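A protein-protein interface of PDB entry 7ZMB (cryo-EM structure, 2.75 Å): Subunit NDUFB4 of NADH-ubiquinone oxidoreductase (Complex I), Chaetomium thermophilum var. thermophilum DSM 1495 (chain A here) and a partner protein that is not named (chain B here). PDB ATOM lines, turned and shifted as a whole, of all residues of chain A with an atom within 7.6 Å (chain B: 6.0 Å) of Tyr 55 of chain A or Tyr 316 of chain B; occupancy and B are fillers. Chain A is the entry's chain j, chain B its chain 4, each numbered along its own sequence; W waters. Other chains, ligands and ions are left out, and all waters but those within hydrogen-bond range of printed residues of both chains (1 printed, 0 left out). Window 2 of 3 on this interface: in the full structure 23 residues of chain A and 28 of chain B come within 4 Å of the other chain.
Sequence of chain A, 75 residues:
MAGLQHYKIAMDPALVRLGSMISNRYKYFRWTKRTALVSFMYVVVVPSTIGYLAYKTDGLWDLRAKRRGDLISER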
ATOM      1  N   PRO A  47     -42.094 -15.123 -23.551  1.00  0.00           N
ATOM      2  CA  PRO A  47     -40.842 -14.427 -23.216  1.00  0.00           C
ATOM      3  C   PRO A  47     -39.916 -15.246 -22.335  1.00  0.00           C
ATOM      4  O   PRO A  47     -38.695 -15.114 -22.446  1.00  0.00           O
ATOM      5  CB  PRO A  47     -41.325 -13.159 -22.501  1.00  0.00           C
ATOM      6  CG  PRO A  47     -42.755 -13.038 -22.835  1.00  0.00           C
ATOM      7  CD  PRO A  47     -43.255 -14.413 -22.989  1.00  0.00           C
ATOM      8  N   THR A  49     -39.551 -18.406 -22.662  1.00  0.00           N
ATOM      9  CA  THR A  49     -38.909 -19.304 -23.612  1.00  0.00           C
ATOM     10  C   THR A  49     -37.745 -18.622 -24.325  1.00  0.00           C
ATOM     11  O   THR A  49     -36.641 -19.173 -24.380  1.00  0.00           O
ATOM     12  CB  THR A  49     -39.938 -19.827 -24.610  1.00  0.00           C
ATOM     13  OG1 THR A  49     -41.090 -20.292 -23.901  1.00  0.00           O
ATOM     14  CG2 THR A  49     -39.353 -20.972 -25.416  1.00  0.00           C
ATOM     15  N   ILE A  50     -37.965 -17.419 -24.877  1.00  0.00           N
ATOM     16  CA  ILE A  50     -36.857 -16.691 -25.506  1.00  0.00           C
ATOM     17  C   ILE A  50     -35.745 -16.435 -24.500  1.00  0.00           C
ATOM     18  O   ILE A  50     -34.569 -16.689 -24.776  1.00  0.00           O
ATOM     19  CB  ILE A  50     -37.330 -15.372 -26.149  1.00  0.00           C
ATOM     20  CG1 ILE A  50     -38.261 -15.598 -27.341  1.00  0.00           C
ATOM     21  CG2 ILE A  50     -36.135 -14.505 -26.523  1.00  0.00           C
ATOM     22  CD1 ILE A  50     -39.697 -15.661 -27.027  1.00  0.00           C
ATOM     23  N   GLY A  51     -36.103 -15.931 -23.318  1.00  0.00           N
ATOM     24  CA  GLY A  51     -35.091 -15.639 -22.320  1.00  0.00           C
ATOM     25  C   GLY A  51     -34.283 -16.861 -21.937  1.00  0.00           C
ATOM     26  O   GLY A  51     -33.063 -16.784 -21.778  1.00  0.00           O
ATOM     27  N   TYR A  52     -34.949 -18.007 -21.792  1.00  0.00           N
ATOM     28  CA  TYR A  52     -34.231 -19.240 -21.495  1.00  0.00           C
ATOM     29  C   TYR A  52     -33.267 -19.602 -22.616  1.00  0.00           C
ATOM     30  O   TYR A  52     -32.136 -20.026 -22.359  1.00  0.00           O
ATOM     31  CB  TYR A  52     -35.211 -20.380 -21.253  1.00  0.00           C
ATOM     32  CG  TYR A  52     -34.522 -21.674 -20.906  1.00  0.00           C
ATOM     33  CD1 TYR A  52     -33.981 -21.874 -19.648  1.00  0.00           C
ATOM     34  CD2 TYR A  52     -34.400 -22.692 -21.839  1.00  0.00           C
ATOM     35  CE1 TYR A  52     -33.345 -23.050 -19.325  1.00  0.00           C
ATOM     36  CE2 TYR A  52     -33.765 -23.873 -21.525  1.00  0.00           C
ATOM     37  CZ  TYR A  52     -33.239 -24.046 -20.266  1.00  0.00           C
ATOM     38  OH  TYR A  52     -32.604 -25.222 -19.946  1.00  0.00           O
ATOM     39  N   LEU A  53     -33.692 -19.449 -23.867  1.00  0.00           N
ATOM     40  CA  LEU A  53     -32.796 -19.758 -24.972  1.00  0.00           C
ATOM     41  C   LEU A  53     -31.670 -18.741 -25.075  1.00  0.00           C
ATOM     42  O   LEU A  53     -30.526 -19.106 -25.362  1.00  0.00           O
ATOM     43  CB  LEU A  53     -33.579 -19.836 -26.277  1.00  0.00           C
ATOM     44  CG  LEU A  53     -34.109 -21.229 -26.605  1.00  0.00           C
ATOM     45  CD1 LEU A  53     -34.693 -21.264 -28.005  1.00  0.00           C
ATOM     46  CD2 LEU A  53     -32.998 -22.245 -26.455  1.00  0.00           C
ATOM     47  N   ALA A  54     -31.967 -17.463 -24.848  1.00  0.00           N
ATOM     48  CA  ALA A  54     -30.919 -16.450 -24.894  1.00  0.00           C
ATOM     49  C   ALA A  54     -29.864 -16.712 -23.833  1.00  0.00           C
ATOM     50  O   ALA A  54     -28.662 -16.639 -24.112  1.00  0.00           O
ATOM     51  CB  ALA A  54     -31.525 -15.058 -24.728  1.00  0.00           C
ATOM     52  N   TYR A  55     -30.299 -17.025 -22.615  1.00  0.00           N
ATOM     53  CA  TYR A  55     -29.370 -17.368 -21.547  1.00  0.00           C
ATOM     54  C   TYR A  55     -28.567 -18.611 -21.894  1.00  0.00           C
ATOM     55  O   TYR A  55     -27.343 -18.641 -21.724  1.00  0.00           O
ATOM     56  CB  TYR A  55     -30.141 -17.566 -20.241  1.00  0.00           C
ATOM     57  CG  TYR A  55     -29.265 -17.629 -19.016  1.00  0.00           C
ATOM     58  CD1 TYR A  55     -28.708 -18.832 -18.600  1.00  0.00           C
ATOM     59  CD2 TYR A  55     -29.010 -16.498 -18.263  1.00  0.00           C
ATOM     60  CE1 TYR A  55     -27.910 -18.899 -17.477  1.00  0.00           C
ATOM     61  CE2 TYR A  55     -28.215 -16.551 -17.140  1.00  0.00           C
ATOM     62  CZ  TYR A  55     -27.666 -17.755 -16.748  1.00  0.00           C
ATOM     63  OH  TYR A  55     -26.873 -17.812 -15.627  1.00  0.00           O
ATOM     64  N   LYS A  56     -29.236 -19.644 -22.402  1.00  0.00           N
ATOM     65  CA  LYS A  56     -28.574 -20.916 -22.653  1.00  0.00           C
ATOM     66  C   LYS A  56     -27.637 -20.883 -23.850  1.00  0.00           C
ATOM     67  O   LYS A  56     -26.836 -21.807 -24.002  1.00  0.00           O
ATOM     68  CB  LYS A  56     -29.614 -22.016 -22.843  1.00  0.00           C
ATOM     69  CG  LYS A  56     -30.210 -22.530 -21.546  1.00  0.00           C
ATOM     70  CD  LYS A  56     -29.129 -23.064 -20.620  1.00  0.00           C
ATOM     71  CE  LYS A  56     -28.658 -24.440 -21.056  1.00  0.00           C
ATOM     72  NZ  LYS A  56     -27.702 -25.033 -20.081  1.00  0.00           N
ATOM     73  N   THR A  57     -27.698 -19.863 -24.696  1.00  0.00           N
ATOM     74  CA  THR A  57     -26.820 -19.776 -25.859  1.00  0.00           C
ATOM     75  C   THR A  57     -26.140 -18.422 -25.918  1.00  0.00           C
ATOM     76  O   THR A  57     -26.078 -17.780 -26.966  1.00  0.00           O
ATOM     77  CB  THR A  57     -27.580 -20.030 -27.158  1.00  0.00           C
ATOM     78  OG1 THR A  57     -28.662 -19.098 -27.274  1.00  0.00           O
ATOM     79  CG2 THR A  57     -28.123 -21.452 -27.195  1.00  0.00           C
ATOM     80  N   ASP A  58     -25.603 -17.972 -24.793  1.00  0.00           N
ATOM     81  CA  ASP A  58     -24.974 -16.661 -24.694  1.00  0.00           C
ATOM     82  C   ASP A  58     -23.469 -16.848 -24.557  1.00  0.00           C
ATOM     83  O   ASP A  58     -23.004 -17.553 -23.656  1.00  0.00           O
ATOM     84  CB  ASP A  58     -25.548 -15.875 -23.518  1.00  0.00           C
ATOM     85  CG  ASP A  58     -25.173 -14.421 -23.556  1.00  0.00           C
ATOM     86  OD1 ASP A  58     -24.352 -14.040 -24.409  1.00  0.00           O
ATOM     87  OD2 ASP A  58     -25.722 -13.644 -22.755  1.00  0.00           O
ATOM     88  N   GLY A  59     -22.716 -16.219 -25.454  1.00  0.00           N
ATOM     89  CA  GLY A  59     -21.303 -16.470 -25.580  1.00  0.00           C
ATOM     90  C   GLY A  59     -20.955 -17.763 -26.277  1.00  0.00           C
ATOM     91  O   GLY A  59     -19.770 -18.101 -26.366  1.00  0.00           O
ATOM     92  N   LEU A  60     -21.947 -18.493 -26.786  1.00  0.00           N
ATOM     93  CA  LEU A  60     -21.701 -19.846 -27.272  1.00  0.00           C
ATOM     94  C   LEU A  60     -21.010 -19.841 -28.628  1.00  0.00           C
ATOM     95  O   LEU A  60     -20.160 -20.694 -28.894  1.00  0.00           O
ATOM     96  CB  LEU A  60     -23.020 -20.620 -27.334  1.00  0.00           C
ATOM     97  CG  LEU A  60     -23.057 -21.993 -28.006  1.00  0.00           C
ATOM     98  CD1 LEU A  60     -21.957 -22.908 -27.479  1.00  0.00           C
ATOM     99  CD2 LEU A  60     -24.418 -22.618 -27.809  1.00  0.00           C
ATOM    100  N   ARG A  75     -17.889 -22.299 -26.254  1.00  0.00           N
ATOM    101  CA  ARG A  75     -18.178 -22.813 -24.924  1.00  0.00           C
ATOM    102  C   ARG A  75     -18.813 -24.197 -25.007  1.00  0.00           C
ATOM    103  O   ARG A  75     -19.481 -24.524 -25.986  1.00  0.00           O
ATOM    104  CB  ARG A  75     -19.093 -21.842 -24.172  1.00  0.00           C
ATOM    105  CG  ARG A  75     -19.512 -22.310 -22.790  1.00  0.00           C
ATOM    106  CD  ARG A  75     -20.267 -21.222 -22.044  1.00  0.00           C
ATOM    107  NE  ARG A  75     -21.161 -20.463 -22.915  1.00  0.00           N
ATOM    108  CZ  ARG A  75     -22.317 -20.919 -23.387  1.00  0.00           C
ATOM    109  NH1 ARG A  75     -23.063 -20.152 -24.169  1.00  0.00           N
ATOM    110  NH2 ARG A  75     -22.731 -22.141 -23.078  1.00  0.00           N
ATOM    111  OXT ARG A  75     -18.667 -25.024 -24.108  1.00  0.00           O
ATOM    112  N   SER B 311     -24.795  -4.784 -17.069  1.00  0.00           N
ATOM    113  CA  SER B 311     -25.357  -4.873 -18.414  1.00  0.00           C
ATOM    114  C   SER B 311     -24.944  -6.162 -19.103  1.00  0.00           C
ATOM    115  O   SER B 311     -25.771  -6.816 -19.745  1.00  0.00           O
ATOM    116  CB  SER B 311     -24.920  -3.668 -19.243  1.00  0.00           C
ATOM    117  OG  SER B 311     -25.378  -3.782 -20.572  1.00  0.00           O
ATOM    118  N   ASN B 313     -24.388  -9.043 -18.056  1.00  0.00           N
ATOM    119  CA  ASN B 313     -25.026 -10.253 -17.562  1.00  0.00           C
ATOM    120  C   ASN B 313     -26.541 -10.225 -17.667  1.00  0.00           C
ATOM    121  O   ASN B 313     -27.168 -11.280 -17.551  1.00  0.00           O
ATOM    122  CB  ASN B 313     -24.627 -10.508 -16.107  1.00  0.00           C
ATOM    123  CG  ASN B 313     -23.243 -11.114 -15.982  1.00  0.00           C
ATOM    124  OD1 ASN B 313     -22.553 -11.318 -16.975  1.00  0.00           O
ATOM    125  ND2 ASN B 313     -22.834 -11.408 -14.756  1.00  0.00           N
ATOM    126  N   LEU B 314     -27.144  -9.064 -17.901  1.00  0.00           N
ATOM    127  CA  LEU B 314     -28.592  -8.944 -17.951  1.00  0.00           C
ATOM    128  C   LEU B 314     -29.121  -8.753 -19.364  1.00  0.00           C
ATOM    129  O   LEU B 314     -30.317  -8.507 -19.540  1.00  0.00           O
ATOM    130  CB  LEU B 314     -29.054  -7.798 -17.057  1.00  0.00           C
ATOM    131  CG  LEU B 314     -28.718  -7.947 -15.579  1.00  0.00           C
ATOM    132  CD1 LEU B 314     -29.635  -7.085 -14.770  1.00  0.00           C
ATOM    133  CD2 LEU B 314     -28.807  -9.396 -15.128  1.00  0.00           C
ATOM    134  N   THR B 315     -28.264  -8.878 -20.373  1.00  0.00           N
ATOM    135  CA  THR B 315     -28.700  -8.661 -21.745  1.00  0.00           C
ATOM    136  C   THR B 315     -29.750  -9.676 -22.175  1.00  0.00           C
ATOM    137  O   THR B 315     -30.629  -9.349 -22.977  1.00  0.00           O
ATOM    138  CB  THR B 315     -27.493  -8.704 -22.682  1.00  0.00           C
ATOM    139  OG1 THR B 315     -26.428  -7.937 -22.108  1.00  0.00           O
ATOM    140  CG2 THR B 315     -27.841  -8.126 -24.036  1.00  0.00           C
ATOM    141  N   TYR B 316     -29.692 -10.898 -21.647  1.00  0.00           N
ATOM    142  CA  TYR B 316     -30.661 -11.904 -22.062  1.00  0.00           C
ATOM    143  C   TYR B 316     -32.073 -11.569 -21.591  1.00  0.00           C
ATOM    144  O   TYR B 316     -33.043 -11.950 -22.255  1.00  0.00           O
ATOM    145  CB  TYR B 316     -30.238 -13.294 -21.591  1.00  0.00           C
ATOM    146  CG  TYR B 316     -30.401 -13.539 -20.119  1.00  0.00           C
ATOM    147  CD1 TYR B 316     -29.569 -12.927 -19.199  1.00  0.00           C
ATOM    148  CD2 TYR B 316     -31.437 -14.325 -19.645  1.00  0.00           C
ATOM    149  CE1 TYR B 316     -29.724 -13.146 -17.855  1.00  0.00           C
ATOM    150  CE2 TYR B 316     -31.612 -14.527 -18.299  1.00  0.00           C
ATOM    151  CZ  TYR B 316     -30.758 -13.938 -17.410  1.00  0.00           C
ATOM    152  OH  TYR B 316     -30.934 -14.155 -16.072  1.00  0.00           O
ATOM    153  N   ILE B 317     -32.214 -10.862 -20.467  1.00  0.00           N
ATOM    154  CA  ILE B 317     -33.515 -10.304 -20.108  1.00  0.00           C
ATOM    155  C   ILE B 317     -33.920  -9.233 -21.109  1.00  0.00           C
ATOM    156  O   ILE B 317     -35.045  -9.223 -21.618  1.00  0.00           O
ATOM    157  CB  ILE B 317     -33.497  -9.723 -18.684  1.00  0.00           C
ATOM    158  CG1 ILE B 317     -33.201 -10.791 -17.636  1.00  0.00           C
ATOM    159  CG2 ILE B 317     -34.790  -9.000 -18.386  1.00  0.00           C
ATOM    160  CD1 ILE B 317     -31.811 -10.735 -17.155  1.00  0.00           C
ATOM    161  N   VAL B 318     -33.003  -8.313 -21.396  1.00  0.00           N
ATOM    162  CA  VAL B 318     -33.313  -7.164 -22.237  1.00  0.00           C
ATOM    163  C   VAL B 318     -33.662  -7.614 -23.644  1.00  0.00           C
ATOM    164  O   VAL B 318     -34.578  -7.079 -24.275  1.00  0.00           O
ATOM    165  CB  VAL B 318     -32.128  -6.179 -22.221  1.00  0.00           C
ATOM    166  CG1 VAL B 318     -32.374  -5.016 -23.159  1.00  0.00           C
ATOM    167  CG2 VAL B 318     -31.890  -5.697 -20.819  1.00  0.00           C
ATOM    168  N   TYR B 319     -32.944  -8.606 -24.156  1.00  0.00           N
ATOM    169  CA  TYR B 319     -33.210  -9.079 -25.504  1.00  0.00           C
ATOM    170  C   TYR B 319     -34.479  -9.913 -25.569  1.00  0.00           C
ATOM    171  O   TYR B 319     -35.142  -9.943 -26.608  1.00  0.00           O
ATOM    172  CB  TYR B 319     -32.004  -9.858 -26.016  1.00  0.00           C
ATOM    173  CG  TYR B 319     -30.894  -8.949 -26.488  1.00  0.00           C
ATOM    174  CD1 TYR B 319     -30.970  -7.577 -26.289  1.00  0.00           C
ATOM    175  CD2 TYR B 319     -29.780  -9.451 -27.129  1.00  0.00           C
ATOM    176  CE1 TYR B 319     -29.973  -6.743 -26.712  1.00  0.00           C
ATOM    177  CE2 TYR B 319     -28.775  -8.620 -27.555  1.00  0.00           C
ATOM    178  CZ  TYR B 319     -28.878  -7.269 -27.343  1.00  0.00           C
ATOM    179  OH  TYR B 319     -27.883  -6.435 -27.769  1.00  0.00           O
ATOM    180  N   ALA B 320     -34.835 -10.589 -24.479  1.00  0.00           N
ATOM    181  CA  ALA B 320     -36.144 -11.221 -24.400  1.00  0.00           C
ATOM    182  C   ALA B 320     -37.245 -10.176 -24.447  1.00  0.00           C
ATOM    183  O   ALA B 320     -38.203 -10.300 -25.215  1.00  0.00           O
ATOM    184  CB  ALA B 320     -36.251 -12.061 -23.129  1.00  0.00           C
ATOM    185  N   ILE B 321     -37.112  -9.120 -23.646  1.00  0.00           N
ATOM    186  CA  ILE B 321     -38.088  -8.037 -23.674  1.00  0.00           C
ATOM    187  C   ILE B 321     -38.079  -7.350 -25.033  1.00  0.00           C
ATOM    188  O   ILE B 321     -39.136  -7.075 -25.608  1.00  0.00           O
ATOM    189  CB  ILE B 321     -37.815  -7.053 -22.522  1.00  0.00           C
ATOM    190  CG1 ILE B 321     -37.919  -7.777 -21.179  1.00  0.00           C
ATOM    191  CG2 ILE B 321     -38.768  -5.876 -22.575  1.00  0.00           C
ATOM    192  CD1 ILE B 321     -37.391  -6.994 -20.005  1.00  0.00           C
ATOM    193  N   ARG B 446     -24.026  -9.929 -30.824  1.00  0.00           N
ATOM    194  CA  ARG B 446     -23.984 -10.067 -29.375  1.00  0.00           C
ATOM    195  C   ARG B 446     -24.761 -11.290 -28.898  1.00  0.00           C
ATOM    196  O   ARG B 446     -24.282 -12.039 -28.043  1.00  0.00           O
ATOM    197  CB  ARG B 446     -24.517  -8.787 -28.718  1.00  0.00           C
ATOM    198  CG  ARG B 446     -24.923  -8.936 -27.273  1.00  0.00           C
ATOM    199  CD  ARG B 446     -23.718  -8.878 -26.366  1.00  0.00           C
ATOM    200  NE  ARG B 446     -23.996  -9.355 -25.014  1.00  0.00           N
ATOM    201  CZ  ARG B 446     -24.040 -10.635 -24.666  1.00  0.00           C
ATOM    202  NH1 ARG B 446     -24.285 -10.972 -23.415  1.00  0.00           N
ATOM    203  NH2 ARG B 446     -23.833 -11.579 -25.569  1.00  0.00           N
ATOM    204  N   LEU B 447     -25.958 -11.505 -29.438  1.00  0.00           N
ATOM    205  CA  LEU B 447     -26.775 -12.675 -29.122  1.00  0.00           C
ATOM    206  C   LEU B 447     -27.461 -13.117 -30.402  1.00  0.00           C
ATOM    207  O   LEU B 447     -28.460 -12.512 -30.819  1.00  0.00           O
ATOM    208  CB  LEU B 447     -27.800 -12.384 -28.029  1.00  0.00           C
ATOM    209  CG  LEU B 447     -27.357 -12.751 -26.615  1.00  0.00           C
ATOM    210  CD1 LEU B 447     -28.323 -12.241 -25.573  1.00  0.00           C
ATOM    211  CD2 LEU B 447     -27.214 -14.256 -26.521  1.00  0.00           C
ATOM    212  N   ILE B 449     -29.544 -15.532 -31.367  1.00  0.00           N
ATOM    213  CA  ILE B 449     -30.961 -15.877 -31.418  1.00  0.00           C
ATOM    214  C   ILE B 449     -31.825 -14.632 -31.249  1.00  0.00           C
ATOM    215  O   ILE B 449     -32.894 -14.516 -31.857  1.00  0.00           O
ATOM    216  CB  ILE B 449     -31.307 -16.956 -30.377  1.00  0.00           C
ATOM    217  CG1 ILE B 449     -31.315 -16.378 -28.966  1.00  0.00           C
ATOM    218  CG2 ILE B 449     -30.323 -18.114 -30.462  1.00  0.00           C
ATOM    219  CD1 ILE B 449     -32.250 -17.097 -28.061  1.00  0.00           C
HETATM  220  O   HOH W   1     -26.583 -11.831 -20.915  1.00  0.00           O
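Of the 13 printed residues of chain B, 5 touch a printed residue of chain A.
Printed residues of chain B that touch a printed residue of chain A: Tyr 316, Ala 320, Arg 446, Leu 447 and Ile 449.
Hydrophobic or aromatic side chains of chain B that line the printed part of chain A: Tyr 316, Ala 320, Leu 447 and Ile 449.
Along chain B the printed residues that touch a printed residue of chain A span positions 316 to 449.
Of the 14 printed residues of chain A, 8 touch a printed residue of chain B.
Hydrophobic or aromatic side chains of chain A within 4 Å of the printed part of chain B: Ile 50, Leu 53, Ala 54 and Tyr 55.
Water W1 lies within hydrogen-bond range of OD2 of Asp 58 of chain A, N of Tyr 316 of chain B, N of Thr 315 of chain B and O of Asn 313 of chain B.
Of the printed residues of chain B, Gly 51 of chain A touches Tyr 316 and Ala 320.
Tyr 55 of chain A touches one residue of chain B.
Lys 56 of chain A touches none of the printed residues of chain B.
Gly 59 of chain A touches none of the printed residues of chain B.
Of the printed residues of chain A, Ala 320 of chain B touches Pro 47, Ile 50 and Gly 51.
Of the printed residues of chain A, Ile 449 of chain B touches Leu 53 (3.5 Å), Ala 54 (3.2 Å) and Thr 57 (3.7 Å).
The nearest residue of chain B that does not touch Tyr 55 of chain A is Asn 313 of chain B (5.4 Å).
O of Asp 58 of chain A is in hydrogen-bond range of NH1 of Arg 75 of chain A.
The backbone carbonyl oxygen (O) of Leu 53 of chain A lies within hydrogen-bond range of the side-chain hydroxyl (OG1) of Thr 57 of chain A, at 2.7 Å.
Among the printed residues, pairs that only touch across the chains: Tyr 55 of chain A with Tyr 316 of chain B (3.2 Å), Ala 54 of chain A with Ile 449 of chain B (3.2 Å), Leu 53 of chain A with Ile 449 of chain B (3.5 Å), Asp 58 of chain A with Leu 447 of chain B (3.6 Å), Gly 51 of chain A with Tyr 316 of chain B (3.6 Å), Ala 54 of chain A with Leu 447 of chain B (3.7 Å), Thr 57 of chain A with Ile 449 of chain B (3.7 Å), Thr 57 of chain A with Leu 447 of chain B (3.7 Å), Ala 54 of chain A with Tyr 316 of chain B (3.8 Å), Gly 51 of chain A with Ala 320 of chain B (3.8 Å), Ile 50 of chain A with Ala 320 of chain B (3.9 Å) and Pro 47 of chain A with Ala 320 of chain B (3.97 Å).
OD1 of Asp 58 of chain A lies within salt-bridge range of NH2 of Arg 446 of chain B.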
